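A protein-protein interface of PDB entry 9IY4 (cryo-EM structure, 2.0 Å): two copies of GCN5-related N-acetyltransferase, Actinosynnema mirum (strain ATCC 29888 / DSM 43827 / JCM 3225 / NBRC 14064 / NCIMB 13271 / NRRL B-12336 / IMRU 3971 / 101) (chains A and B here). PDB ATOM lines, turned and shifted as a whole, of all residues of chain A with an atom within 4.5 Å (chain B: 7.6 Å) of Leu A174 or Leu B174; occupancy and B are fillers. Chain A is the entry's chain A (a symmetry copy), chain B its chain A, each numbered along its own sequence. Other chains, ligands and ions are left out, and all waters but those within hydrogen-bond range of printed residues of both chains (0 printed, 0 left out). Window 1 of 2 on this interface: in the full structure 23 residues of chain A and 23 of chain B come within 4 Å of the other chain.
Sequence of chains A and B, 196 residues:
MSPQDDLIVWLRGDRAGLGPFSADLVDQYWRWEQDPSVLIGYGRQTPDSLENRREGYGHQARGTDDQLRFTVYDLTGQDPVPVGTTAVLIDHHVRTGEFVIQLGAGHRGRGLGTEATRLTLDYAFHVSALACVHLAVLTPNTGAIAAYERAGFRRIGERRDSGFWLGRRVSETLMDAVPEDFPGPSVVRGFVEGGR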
ATOM      1  N   LEU A 135     -35.208  17.466 -10.163  1.00  0.00           N
ATOM      2  CA  LEU A 135     -35.861  17.914 -11.380  1.00  0.00           C
ATOM      3  C   LEU A 135     -34.812  18.406 -12.364  1.00  0.00           C
ATOM      4  O   LEU A 135     -33.687  18.740 -11.989  1.00  0.00           O
ATOM      5  CB  LEU A 135     -36.891  19.015 -11.094  1.00  0.00           C
ATOM      6  CG  LEU A 135     -36.457  20.335 -10.448  1.00  0.00           C
ATOM      7  CD1 LEU A 135     -35.864  21.322 -11.435  1.00  0.00           C
ATOM      8  CD2 LEU A 135     -37.621  20.954  -9.721  1.00  0.00           C
ATOM      9  N   ALA A 136     -35.204  18.449 -13.633  1.00  0.00           N
ATOM     10  CA  ALA A 136     -34.411  19.051 -14.693  1.00  0.00           C
ATOM     11  C   ALA A 136     -35.257  20.107 -15.385  1.00  0.00           C
ATOM     12  O   ALA A 136     -36.375  19.823 -15.825  1.00  0.00           O
ATOM     13  CB  ALA A 136     -33.937  18.002 -15.696  1.00  0.00           C
ATOM     14  N   ARG A 154     -32.974  23.152  -4.350  1.00  0.00           N
ATOM     15  CA  ARG A 154     -31.694  23.843  -4.371  1.00  0.00           C
ATOM     16  C   ARG A 154     -30.965  23.502  -5.661  1.00  0.00           C
ATOM     17  O   ARG A 154     -31.095  22.397  -6.189  1.00  0.00           O
ATOM     18  CB  ARG A 154     -30.819  23.465  -3.172  1.00  0.00           C
ATOM     19  CG  ARG A 154     -31.419  23.806  -1.826  1.00  0.00           C
ATOM     20  CD  ARG A 154     -31.467  25.297  -1.581  1.00  0.00           C
ATOM     21  NE  ARG A 154     -31.989  25.596  -0.255  1.00  0.00           N
ATOM     22  CZ  ARG A 154     -33.271  25.803   0.016  1.00  0.00           C
ATOM     23  NH1 ARG A 154     -34.192  25.776  -0.933  1.00  0.00           N
ATOM     24  NH2 ARG A 154     -33.638  26.046   1.271  1.00  0.00           N
ATOM     25  N   ARG A 155     -30.188  24.458  -6.157  1.00  0.00           N
ATOM     26  CA  ARG A 155     -29.505  24.289  -7.431  1.00  0.00           C
ATOM     27  C   ARG A 155     -28.315  23.346  -7.297  1.00  0.00           C
ATOM     28  O   ARG A 155     -27.503  23.479  -6.378  1.00  0.00           O
ATOM     29  CB  ARG A 155     -29.047  25.646  -7.960  1.00  0.00           C
ATOM     30  CG  ARG A 155     -28.286  25.581  -9.265  1.00  0.00           C
ATOM     31  CD  ARG A 155     -27.915  26.966  -9.765  1.00  0.00           C
ATOM     32  NE  ARG A 155     -29.056  27.667 -10.342  1.00  0.00           N
ATOM     33  CZ  ARG A 155     -29.698  28.667  -9.756  1.00  0.00           C
ATOM     34  NH1 ARG A 155     -29.356  29.097  -8.553  1.00  0.00           N
ATOM     35  NH2 ARG A 155     -30.707  29.251 -10.393  1.00  0.00           N
ATOM     36  N   ILE A 156     -28.214  22.393  -8.219  1.00  0.00           N
ATOM     37  CA  ILE A 156     -27.045  21.524  -8.311  1.00  0.00           C
ATOM     38  C   ILE A 156     -26.012  22.098  -9.267  1.00  0.00           C
ATOM     39  O   ILE A 156     -24.847  22.280  -8.911  1.00  0.00           O
ATOM     40  CB  ILE A 156     -27.464  20.109  -8.757  1.00  0.00           C
ATOM     41  CG1 ILE A 156     -28.406  19.461  -7.750  1.00  0.00           C
ATOM     42  CG2 ILE A 156     -26.246  19.242  -8.968  1.00  0.00           C
ATOM     43  CD1 ILE A 156     -29.064  18.211  -8.288  1.00  0.00           C
ATOM     44  N   GLY A 157     -26.436  22.390 -10.490  1.00  0.00           N
ATOM     45  CA  GLY A 157     -25.537  22.863 -11.518  1.00  0.00           C
ATOM     46  C   GLY A 157     -26.245  22.855 -12.858  1.00  0.00           C
ATOM     47  O   GLY A 157     -27.444  22.586 -12.940  1.00  0.00           O
ATOM     48  N   ARG A 159     -26.329  21.413 -16.810  1.00  0.00           N
ATOM     49  CA  ARG A 159     -25.952  20.393 -17.781  1.00  0.00           C
ATOM     50  C   ARG A 159     -25.866  21.067 -19.145  1.00  0.00           C
ATOM     51  O   ARG A 159     -26.892  21.411 -19.738  1.00  0.00           O
ATOM     52  CB  ARG A 159     -26.966  19.255 -17.791  1.00  0.00           C
ATOM     53  CG  ARG A 159     -26.647  18.142 -18.755  1.00  0.00           C
ATOM     54  CD  ARG A 159     -27.793  17.157 -18.829  1.00  0.00           C
ATOM     55  NE  ARG A 159     -27.951  16.395 -17.600  1.00  0.00           N
ATOM     56  CZ  ARG A 159     -29.079  15.806 -17.229  1.00  0.00           C
ATOM     57  NH1 ARG A 159     -30.176  15.896 -17.960  1.00  0.00           N
ATOM     58  NH2 ARG A 159     -29.106  15.115 -16.094  1.00  0.00           N
ATOM     59  N   GLU A 172     -29.586  23.068 -19.224  1.00  0.00           N
ATOM     60  CA  GLU A 172     -30.692  22.872 -18.305  1.00  0.00           C
ATOM     61  C   GLU A 172     -30.166  22.797 -16.879  1.00  0.00           C
ATOM     62  O   GLU A 172     -29.074  22.285 -16.627  1.00  0.00           O
ATOM     63  CB  GLU A 172     -31.500  21.617 -18.657  1.00  0.00           C
ATOM     64  CG  GLU A 172     -30.824  20.308 -18.381  1.00  0.00           C
ATOM     65  CD  GLU A 172     -31.655  19.132 -18.854  1.00  0.00           C
ATOM     66  OE1 GLU A 172     -32.763  19.364 -19.381  1.00  0.00           O
ATOM     67  OE2 GLU A 172     -31.200  17.979 -18.705  1.00  0.00           O
ATOM     68  N   THR A 173     -30.950  23.339 -15.953  1.00  0.00           N
ATOM     69  CA  THR A 173     -30.559  23.436 -14.555  1.00  0.00           C
ATOM     70  C   THR A 173     -31.068  22.221 -13.795  1.00  0.00           C
ATOM     71  O   THR A 173     -32.236  21.846 -13.922  1.00  0.00           O
ATOM     72  CB  THR A 173     -31.110  24.719 -13.930  1.00  0.00           C
ATOM     73  OG1 THR A 173     -30.593  25.849 -14.634  1.00  0.00           O
ATOM     74  CG2 THR A 173     -30.713  24.821 -12.475  1.00  0.00           C
ATOM     75  N   LEU A 174     -30.189  21.607 -13.013  1.00  0.00           N
ATOM     76  CA  LEU A 174     -30.535  20.458 -12.191  1.00  0.00           C
ATOM     77  C   LEU A 174     -30.741  20.925 -10.758  1.00  0.00           C
ATOM     78  O   LEU A 174     -29.912  21.660 -10.217  1.00  0.00           O
ATOM     79  CB  LEU A 174     -29.436  19.399 -12.256  1.00  0.00           C
ATOM     80  CG  LEU A 174     -29.017  18.965 -13.659  1.00  0.00           C
ATOM     81  CD1 LEU A 174     -27.903  17.950 -13.585  1.00  0.00           C
ATOM     82  CD2 LEU A 174     -30.194  18.411 -14.425  1.00  0.00           C
ATOM     83  N   MET A 175     -31.850  20.512 -10.153  1.00  0.00           N
ATOM     84  CA  MET A 175     -32.186  20.933  -8.803  1.00  0.00           C
ATOM     85  C   MET A 175     -32.639  19.722  -8.004  1.00  0.00           C
ATOM     86  O   MET A 175     -33.106  18.730  -8.560  1.00  0.00           O
ATOM     87  CB  MET A 175     -33.276  22.010  -8.805  1.00  0.00           C
ATOM     88  CG  MET A 175     -32.979  23.184  -9.713  1.00  0.00           C
ATOM     89  SD  MET A 175     -34.242  24.456  -9.656  1.00  0.00           S
ATOM     90  CE  MET A 175     -33.866  25.213  -8.084  1.00  0.00           C
ATOM     91  N   HIS B 134     -23.848  12.714 -20.779  1.00  0.00           N
ATOM     92  CA  HIS B 134     -23.853  12.937 -19.344  1.00  0.00           C
ATOM     93  C   HIS B 134     -23.936  11.605 -18.614  1.00  0.00           C
ATOM     94  O   HIS B 134     -24.280  10.574 -19.194  1.00  0.00           O
ATOM     95  CB  HIS B 134     -25.016  13.839 -18.915  1.00  0.00           C
ATOM     96  CG  HIS B 134     -26.361  13.282 -19.247  1.00  0.00           C
ATOM     97  ND1 HIS B 134     -27.054  12.454 -18.394  1.00  0.00           N
ATOM     98  CD2 HIS B 134     -27.150  13.446 -20.334  1.00  0.00           C
ATOM     99  CE1 HIS B 134     -28.203  12.117 -18.948  1.00  0.00           C
ATOM    100  NE2 HIS B 134     -28.288  12.708 -20.124  1.00  0.00           N
ATOM    101  N   LEU B 135     -23.606  11.640 -17.325  1.00  0.00           N
ATOM    102  CA  LEU B 135     -23.579  10.438 -16.509  1.00  0.00           C
ATOM    103  C   LEU B 135     -23.922  10.796 -15.072  1.00  0.00           C
ATOM    104  O   LEU B 135     -23.810  11.950 -14.654  1.00  0.00           O
ATOM    105  CB  LEU B 135     -22.215   9.739 -16.581  1.00  0.00           C
ATOM    106  CG  LEU B 135     -20.944  10.469 -16.133  1.00  0.00           C
ATOM    107  CD1 LEU B 135     -20.734  10.448 -14.631  1.00  0.00           C
ATOM    108  CD2 LEU B 135     -19.747   9.890 -16.839  1.00  0.00           C
ATOM    109  N   ALA B 136     -24.337   9.781 -14.322  1.00  0.00           N
ATOM    110  CA  ALA B 136     -24.544   9.884 -12.886  1.00  0.00           C
ATOM    111  C   ALA B 136     -23.713   8.811 -12.203  1.00  0.00           C
ATOM    112  O   ALA B 136     -23.813   7.629 -12.545  1.00  0.00           O
ATOM    113  CB  ALA B 136     -26.020   9.728 -12.525  1.00  0.00           C
ATOM    114  N   VAL B 137     -22.902   9.223 -11.235  1.00  0.00           N
ATOM    115  CA  VAL B 137     -21.951   8.343 -10.570  1.00  0.00           C
ATOM    116  C   VAL B 137     -21.974   8.619  -9.073  1.00  0.00           C
ATOM    117  O   VAL B 137     -22.013   9.777  -8.644  1.00  0.00           O
ATOM    118  CB  VAL B 137     -20.537   8.511 -11.166  1.00  0.00           C
ATOM    119  CG1 VAL B 137     -20.028   9.885 -10.912  1.00  0.00           C
ATOM    120  CG2 VAL B 137     -19.582   7.524 -10.551  1.00  0.00           C
ATOM    121  N   LEU B 138     -21.980   7.551  -8.278  1.00  0.00           N
ATOM    122  CA  LEU B 138     -21.955   7.699  -6.830  1.00  0.00           C
ATOM    123  C   LEU B 138     -20.671   8.387  -6.390  1.00  0.00           C
ATOM    124  O   LEU B 138     -19.581   8.074  -6.873  1.00  0.00           O
ATOM    125  CB  LEU B 138     -22.091   6.337  -6.153  1.00  0.00           C
ATOM    126  CG  LEU B 138     -23.413   5.596  -6.363  1.00  0.00           C
ATOM    127  CD1 LEU B 138     -23.335   4.201  -5.797  1.00  0.00           C
ATOM    128  CD2 LEU B 138     -24.555   6.352  -5.717  1.00  0.00           C
ATOM    129  N   THR B 139     -20.812   9.337  -5.470  1.00  0.00           N
ATOM    130  CA  THR B 139     -19.683  10.176  -5.078  1.00  0.00           C
ATOM    131  C   THR B 139     -18.491   9.395  -4.531  1.00  0.00           C
ATOM    132  O   THR B 139     -17.355   9.725  -4.913  1.00  0.00           O
ATOM    133  CB  THR B 139     -20.156  11.226  -4.066  1.00  0.00           C
ATOM    134  OG1 THR B 139     -21.113  12.086  -4.687  1.00  0.00           O
ATOM    135  CG2 THR B 139     -18.993  12.068  -3.587  1.00  0.00           C
ATOM    136  N   ILE B 145     -14.651   8.715 -11.049  1.00  0.00           N
ATOM    137  CA  ILE B 145     -14.611  10.168 -11.199  1.00  0.00           C
ATOM    138  C   ILE B 145     -13.359  10.591 -11.954  1.00  0.00           C
ATOM    139  O   ILE B 145     -13.423  11.364 -12.917  1.00  0.00           O
ATOM    140  CB  ILE B 145     -14.678  10.856  -9.824  1.00  0.00           C
ATOM    141  CG1 ILE B 145     -16.014  10.598  -9.141  1.00  0.00           C
ATOM    142  CG2 ILE B 145     -14.470  12.347  -9.981  1.00  0.00           C
ATOM    143  CD1 ILE B 145     -17.142  11.226  -9.844  1.00  0.00           C
ATOM    144  N   PHE B 153     -15.137  14.295 -19.398  1.00  0.00           N
ATOM    145  CA  PHE B 153     -16.307  14.757 -18.668  1.00  0.00           C
ATOM    146  C   PHE B 153     -15.918  15.864 -17.693  1.00  0.00           C
ATOM    147  O   PHE B 153     -14.782  15.938 -17.221  1.00  0.00           O
ATOM    148  CB  PHE B 153     -16.959  13.604 -17.909  1.00  0.00           C
ATOM    149  CG  PHE B 153     -17.748  12.668 -18.775  1.00  0.00           C
ATOM    150  CD1 PHE B 153     -17.126  11.623 -19.424  1.00  0.00           C
ATOM    151  CD2 PHE B 153     -19.107  12.826 -18.934  1.00  0.00           C
ATOM    152  CE1 PHE B 153     -17.845  10.755 -20.206  1.00  0.00           C
ATOM    153  CE2 PHE B 153     -19.828  11.962 -19.725  1.00  0.00           C
ATOM    154  CZ  PHE B 153     -19.196  10.924 -20.357  1.00  0.00           C
ATOM    155  N   ARG B 154     -16.881  16.728 -17.389  1.00  0.00           N
ATOM    156  CA  ARG B 154     -16.694  17.802 -16.427  1.00  0.00           C
ATOM    157  C   ARG B 154     -17.779  17.715 -15.366  1.00  0.00           C
ATOM    158  O   ARG B 154     -18.906  17.307 -15.645  1.00  0.00           O
ATOM    159  CB  ARG B 154     -16.736  19.182 -17.092  1.00  0.00           C
ATOM    160  CG  ARG B 154     -15.664  19.408 -18.135  1.00  0.00           C
ATOM    161  CD  ARG B 154     -14.286  19.518 -17.526  1.00  0.00           C
ATOM    162  NE  ARG B 154     -13.281  19.798 -18.543  1.00  0.00           N
ATOM    163  CZ  ARG B 154     -12.600  18.868 -19.200  1.00  0.00           C
ATOM    164  NH1 ARG B 154     -12.773  17.580 -18.952  1.00  0.00           N
ATOM    165  NH2 ARG B 154     -11.723  19.240 -20.127  1.00  0.00           N
ATOM    166  N   ARG B 155     -17.430  18.113 -14.147  1.00  0.00           N
ATOM    167  CA  ARG B 155     -18.349  17.997 -13.025  1.00  0.00           C
ATOM    168  C   ARG B 155     -19.440  19.060 -13.095  1.00  0.00           C
ATOM    169  O   ARG B 155     -19.160  20.241 -13.313  1.00  0.00           O
ATOM    170  CB  ARG B 155     -17.582  18.115 -11.710  1.00  0.00           C
ATOM    171  CG  ARG B 155     -18.452  18.049 -10.474  1.00  0.00           C
ATOM    172  CD  ARG B 155     -17.622  18.108  -9.204  1.00  0.00           C
ATOM    173  NE  ARG B 155     -16.949  16.845  -8.927  1.00  0.00           N
ATOM    174  CZ  ARG B 155     -15.651  16.633  -9.092  1.00  0.00           C
ATOM    175  NH1 ARG B 155     -14.851  17.576  -9.563  1.00  0.00           N
ATOM    176  NH2 ARG B 155     -15.142  15.447  -8.776  1.00  0.00           N
ATOM    177  N   ILE B 156     -20.686  18.635 -12.908  1.00  0.00           N
ATOM    178  CA  ILE B 156     -21.810  19.559 -12.787  1.00  0.00           C
ATOM    179  C   ILE B 156     -22.066  19.919 -11.332  1.00  0.00           C
ATOM    180  O   ILE B 156     -22.103  21.094 -10.965  1.00  0.00           O
ATOM    181  CB  ILE B 156     -23.076  18.948 -13.422  1.00  0.00           C
ATOM    182  CG1 ILE B 156     -22.886  18.691 -14.912  1.00  0.00           C
ATOM    183  CG2 ILE B 156     -24.265  19.849 -13.193  1.00  0.00           C
ATOM    184  CD1 ILE B 156     -23.981  17.832 -15.499  1.00  0.00           C
ATOM    185  N   GLY B 157     -22.242  18.906 -10.495  1.00  0.00           N
ATOM    186  CA  GLY B 157     -22.575  19.113  -9.103  1.00  0.00           C
ATOM    187  C   GLY B 157     -22.971  17.794  -8.472  1.00  0.00           C
ATOM    188  O   GLY B 157     -22.875  16.737  -9.097  1.00  0.00           O
ATOM    189  N   GLU B 158     -23.430  17.879  -7.229  1.00  0.00           N
ATOM    190  CA  GLU B 158     -23.795  16.706  -6.447  1.00  0.00           C
ATOM    191  C   GLU B 158     -25.292  16.696  -6.178  1.00  0.00           C
ATOM    192  O   GLU B 158     -25.847  17.687  -5.695  1.00  0.00           O
ATOM    193  CB  GLU B 158     -23.028  16.673  -5.126  1.00  0.00           C
ATOM    194  CG  GLU B 158     -21.635  16.095  -5.240  1.00  0.00           C
ATOM    195  CD  GLU B 158     -20.747  16.489  -4.080  1.00  0.00           C
ATOM    196  OE1 GLU B 158     -19.509  16.460  -4.238  1.00  0.00           O
ATOM    197  OE2 GLU B 158     -21.287  16.826  -3.006  1.00  0.00           O
ATOM    198  N   ARG B 159     -25.934  15.571  -6.475  1.00  0.00           N
ATOM    199  CA  ARG B 159     -27.342  15.352  -6.165  1.00  0.00           C
ATOM    200  C   ARG B 159     -27.412  14.696  -4.791  1.00  0.00           C
ATOM    201  O   ARG B 159     -27.082  13.516  -4.644  1.00  0.00           O
ATOM    202  CB  ARG B 159     -27.999  14.479  -7.228  1.00  0.00           C
ATOM    203  CG  ARG B 159     -29.465  14.214  -6.999  1.00  0.00           C
ATOM    204  CD  ARG B 159     -29.983  13.197  -7.992  1.00  0.00           C
ATOM    205  NE  ARG B 159     -30.025  13.718  -9.350  1.00  0.00           N
ATOM    206  CZ  ARG B 159     -30.015  12.962 -10.438  1.00  0.00           C
ATOM    207  NH1 ARG B 159     -29.938  11.646 -10.362  1.00  0.00           N
ATOM    208  NH2 ARG B 159     -30.079  13.544 -11.632  1.00  0.00           N
ATOM    209  N   SER B 162     -29.034  10.545  -2.882  1.00  0.00           N
ATOM    210  CA  SER B 162     -29.701   9.922  -4.016  1.00  0.00           C
ATOM    211  C   SER B 162     -29.107   8.562  -4.362  1.00  0.00           C
ATOM    212  O   SER B 162     -29.288   8.082  -5.483  1.00  0.00           O
ATOM    213  CB  SER B 162     -29.653  10.838  -5.236  1.00  0.00           C
ATOM    214  OG  SER B 162     -28.325  11.002  -5.681  1.00  0.00           O
ATOM    215  N   SER B 171     -24.431  11.026  -1.726  1.00  0.00           N
ATOM    216  CA  SER B 171     -24.793  11.766  -2.921  1.00  0.00           C
ATOM    217  C   SER B 171     -24.176  11.122  -4.158  1.00  0.00           C
ATOM    218  O   SER B 171     -23.293  10.268  -4.074  1.00  0.00           O
ATOM    219  CB  SER B 171     -24.340  13.219  -2.812  1.00  0.00           C
ATOM    220  OG  SER B 171     -22.930  13.307  -2.815  1.00  0.00           O
ATOM    221  N   GLU B 172     -24.647  11.547  -5.324  1.00  0.00           N
ATOM    222  CA  GLU B 172     -24.067  11.110  -6.581  1.00  0.00           C
ATOM    223  C   GLU B 172     -23.648  12.321  -7.401  1.00  0.00           C
ATOM    224  O   GLU B 172     -24.294  13.370  -7.367  1.00  0.00           O
ATOM    225  CB  GLU B 172     -25.039  10.224  -7.371  1.00  0.00           C
ATOM    226  CG  GLU B 172     -26.220  10.926  -7.971  1.00  0.00           C
ATOM    227  CD  GLU B 172     -27.172   9.958  -8.642  1.00  0.00           C
ATOM    228  OE1 GLU B 172     -26.881   8.743  -8.639  1.00  0.00           O
ATOM    229  OE2 GLU B 172     -28.212  10.407  -9.167  1.00  0.00           O
ATOM    230  N   THR B 173     -22.540  12.169  -8.119  1.00  0.00           N
ATOM    231  CA  THR B 173     -21.949  13.253  -8.887  1.00  0.00           C
ATOM    232  C   THR B 173     -22.478  13.221 -10.313  1.00  0.00           C
ATOM    233  O   THR B 173     -22.499  12.165 -10.949  1.00  0.00           O
ATOM    234  CB  THR B 173     -20.423  13.143  -8.887  1.00  0.00           C
ATOM    235  OG1 THR B 173     -19.943  13.212  -7.543  1.00  0.00           O
ATOM    236  CG2 THR B 173     -19.803  14.264  -9.689  1.00  0.00           C
ATOM    237  N   LEU B 174     -22.907  14.375 -10.807  1.00  0.00           N
ATOM    238  CA  LEU B 174     -23.401  14.514 -12.167  1.00  0.00           C
ATOM    239  C   LEU B 174     -22.303  15.120 -13.028  1.00  0.00           C
ATOM    240  O   LEU B 174     -21.690  16.119 -12.644  1.00  0.00           O
ATOM    241  CB  LEU B 174     -24.652  15.391 -12.200  1.00  0.00           C
ATOM    242  CG  LEU B 174     -25.772  14.981 -11.246  1.00  0.00           C
ATOM    243  CD1 LEU B 174     -26.928  15.946 -11.347  1.00  0.00           C
ATOM    244  CD2 LEU B 174     -26.230  13.569 -11.529  1.00  0.00           C
ATOM    245  N   MET B 175     -22.046  14.509 -14.179  1.00  0.00           N
ATOM    246  CA  MET B 175     -20.985  14.960 -15.064  1.00  0.00           C
ATOM    247  C   MET B 175     -21.509  14.995 -16.490  1.00  0.00           C
ATOM    248  O   MET B 175     -22.454  14.290 -16.840  1.00  0.00           O
ATOM    249  CB  MET B 175     -19.752  14.055 -14.971  1.00  0.00           C
ATOM    250  CG  MET B 175     -19.261  13.828 -13.557  1.00  0.00           C
ATOM    251  SD  MET B 175     -17.785  12.812 -13.477  1.00  0.00           S
ATOM    252  CE  MET B 175     -16.555  13.986 -14.019  1.00  0.00           C
ATOM    253  N   ASP B 176     -20.890  15.836 -17.314  1.00  0.00           N
ATOM    254  CA  ASP B 176     -21.270  15.929 -18.716  1.00  0.00           C
ATOM    255  C   ASP B 176     -20.046  16.256 -19.558  1.00  0.00           C
ATOM    256  O   ASP B 176     -19.025  16.726 -19.057  1.00  0.00           O
ATOM    257  CB  ASP B 176     -22.393  16.955 -18.932  1.00  0.00           C
ATOM    258  CG  ASP B 176     -22.029  18.350 -18.465  1.00  0.00           C
ATOM    259  OD1 ASP B 176     -20.839  18.648 -18.251  1.00  0.00           O
ATOM    260  OD2 ASP B 176     -22.954  19.170 -18.316  1.00  0.00           O
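Hydrophobic or aromatic side chains of chain A that line the printed part of chain B: Ile A156 and Leu A174.
Printed residues of chain B that touch a printed residue of chain A: His B134, Ile B156, Gly B157, Glu B158, Arg B159, Leu B174 and Asp B176.
The side-chain carboxylate (OE2) of Glu A172 is in salt-bridge range of the guanidinium group (NH1) of Arg A159, 2.4 Å away.
The backbone carbonyl oxygen (O) of Arg B159 lies within hydrogen-bond range of the side-chain hydroxyl (OG) of Ser B162 (3.0 Å).
The backbone carbonyl oxygen of Gly B157 sits at hydrogen-bond distance from the backbone NH of Leu B174 (2.9 Å).
The backbone carbonyl oxygen of Asp B176 sits at hydrogen-bond distance from the backbone NH of Arg B154, at 2.7 Å.
N of Ile B156 sits at hydrogen-bond distance from O of Leu B174 (2.7 Å).
The backbone NH of Ile A156 is in hydrogen-bond range of the backbone carbonyl oxygen of Leu A174 (2.7 Å).
Among the printed residues, pairs that only touch across the chains: Leu A174 with Leu B174 (3.2 Å), Arg A159 with Asp B176 (3.3 Å), Ile A156 with Glu B158 (3.6 Å), Ile A156 with Gly B157 (3.6 Å), Gly A157 with Ile B156 (3.6 Å), Ile A156 with Ile B156 (3.6 Å), Arg A159 with His B134 (3.9 Å), Ile A156 with Arg B159 (3.96 Å) and Arg A159 with Ile B156 (3.96 Å).
Leu A174 touches one residue of chain B.
Of the printed residues of chain A, Leu B174 touches Leu A174 (3.2 Å).
Of the printed residues of chain A, Arg B159 touches Ile A156.
Of the printed residues of chain A, His B134 touches Arg A159.
Ser B171 touches none of the printed residues of chain A.
Arg A155 touches none of the printed residues of chain B.
The nearest residue of chain B that does not touch Leu A174 is Ile B156 (4.1 Å).
The nearest printed residue of chain A that does not touch Ile B156 is Leu A174 (4.1 Å).
Ile B156 touches its own counterpart, Ile A156.
Ile A156 touches Gly B157, and with the chains exchanged Gly A157 touches Ile B156.
Ile A156 touches Arg B159, and with the chains exchanged Arg A159 touches Ile B156.
Leu B174 touches its own counterpart, Leu A174.
11 positions are printed for both chains.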
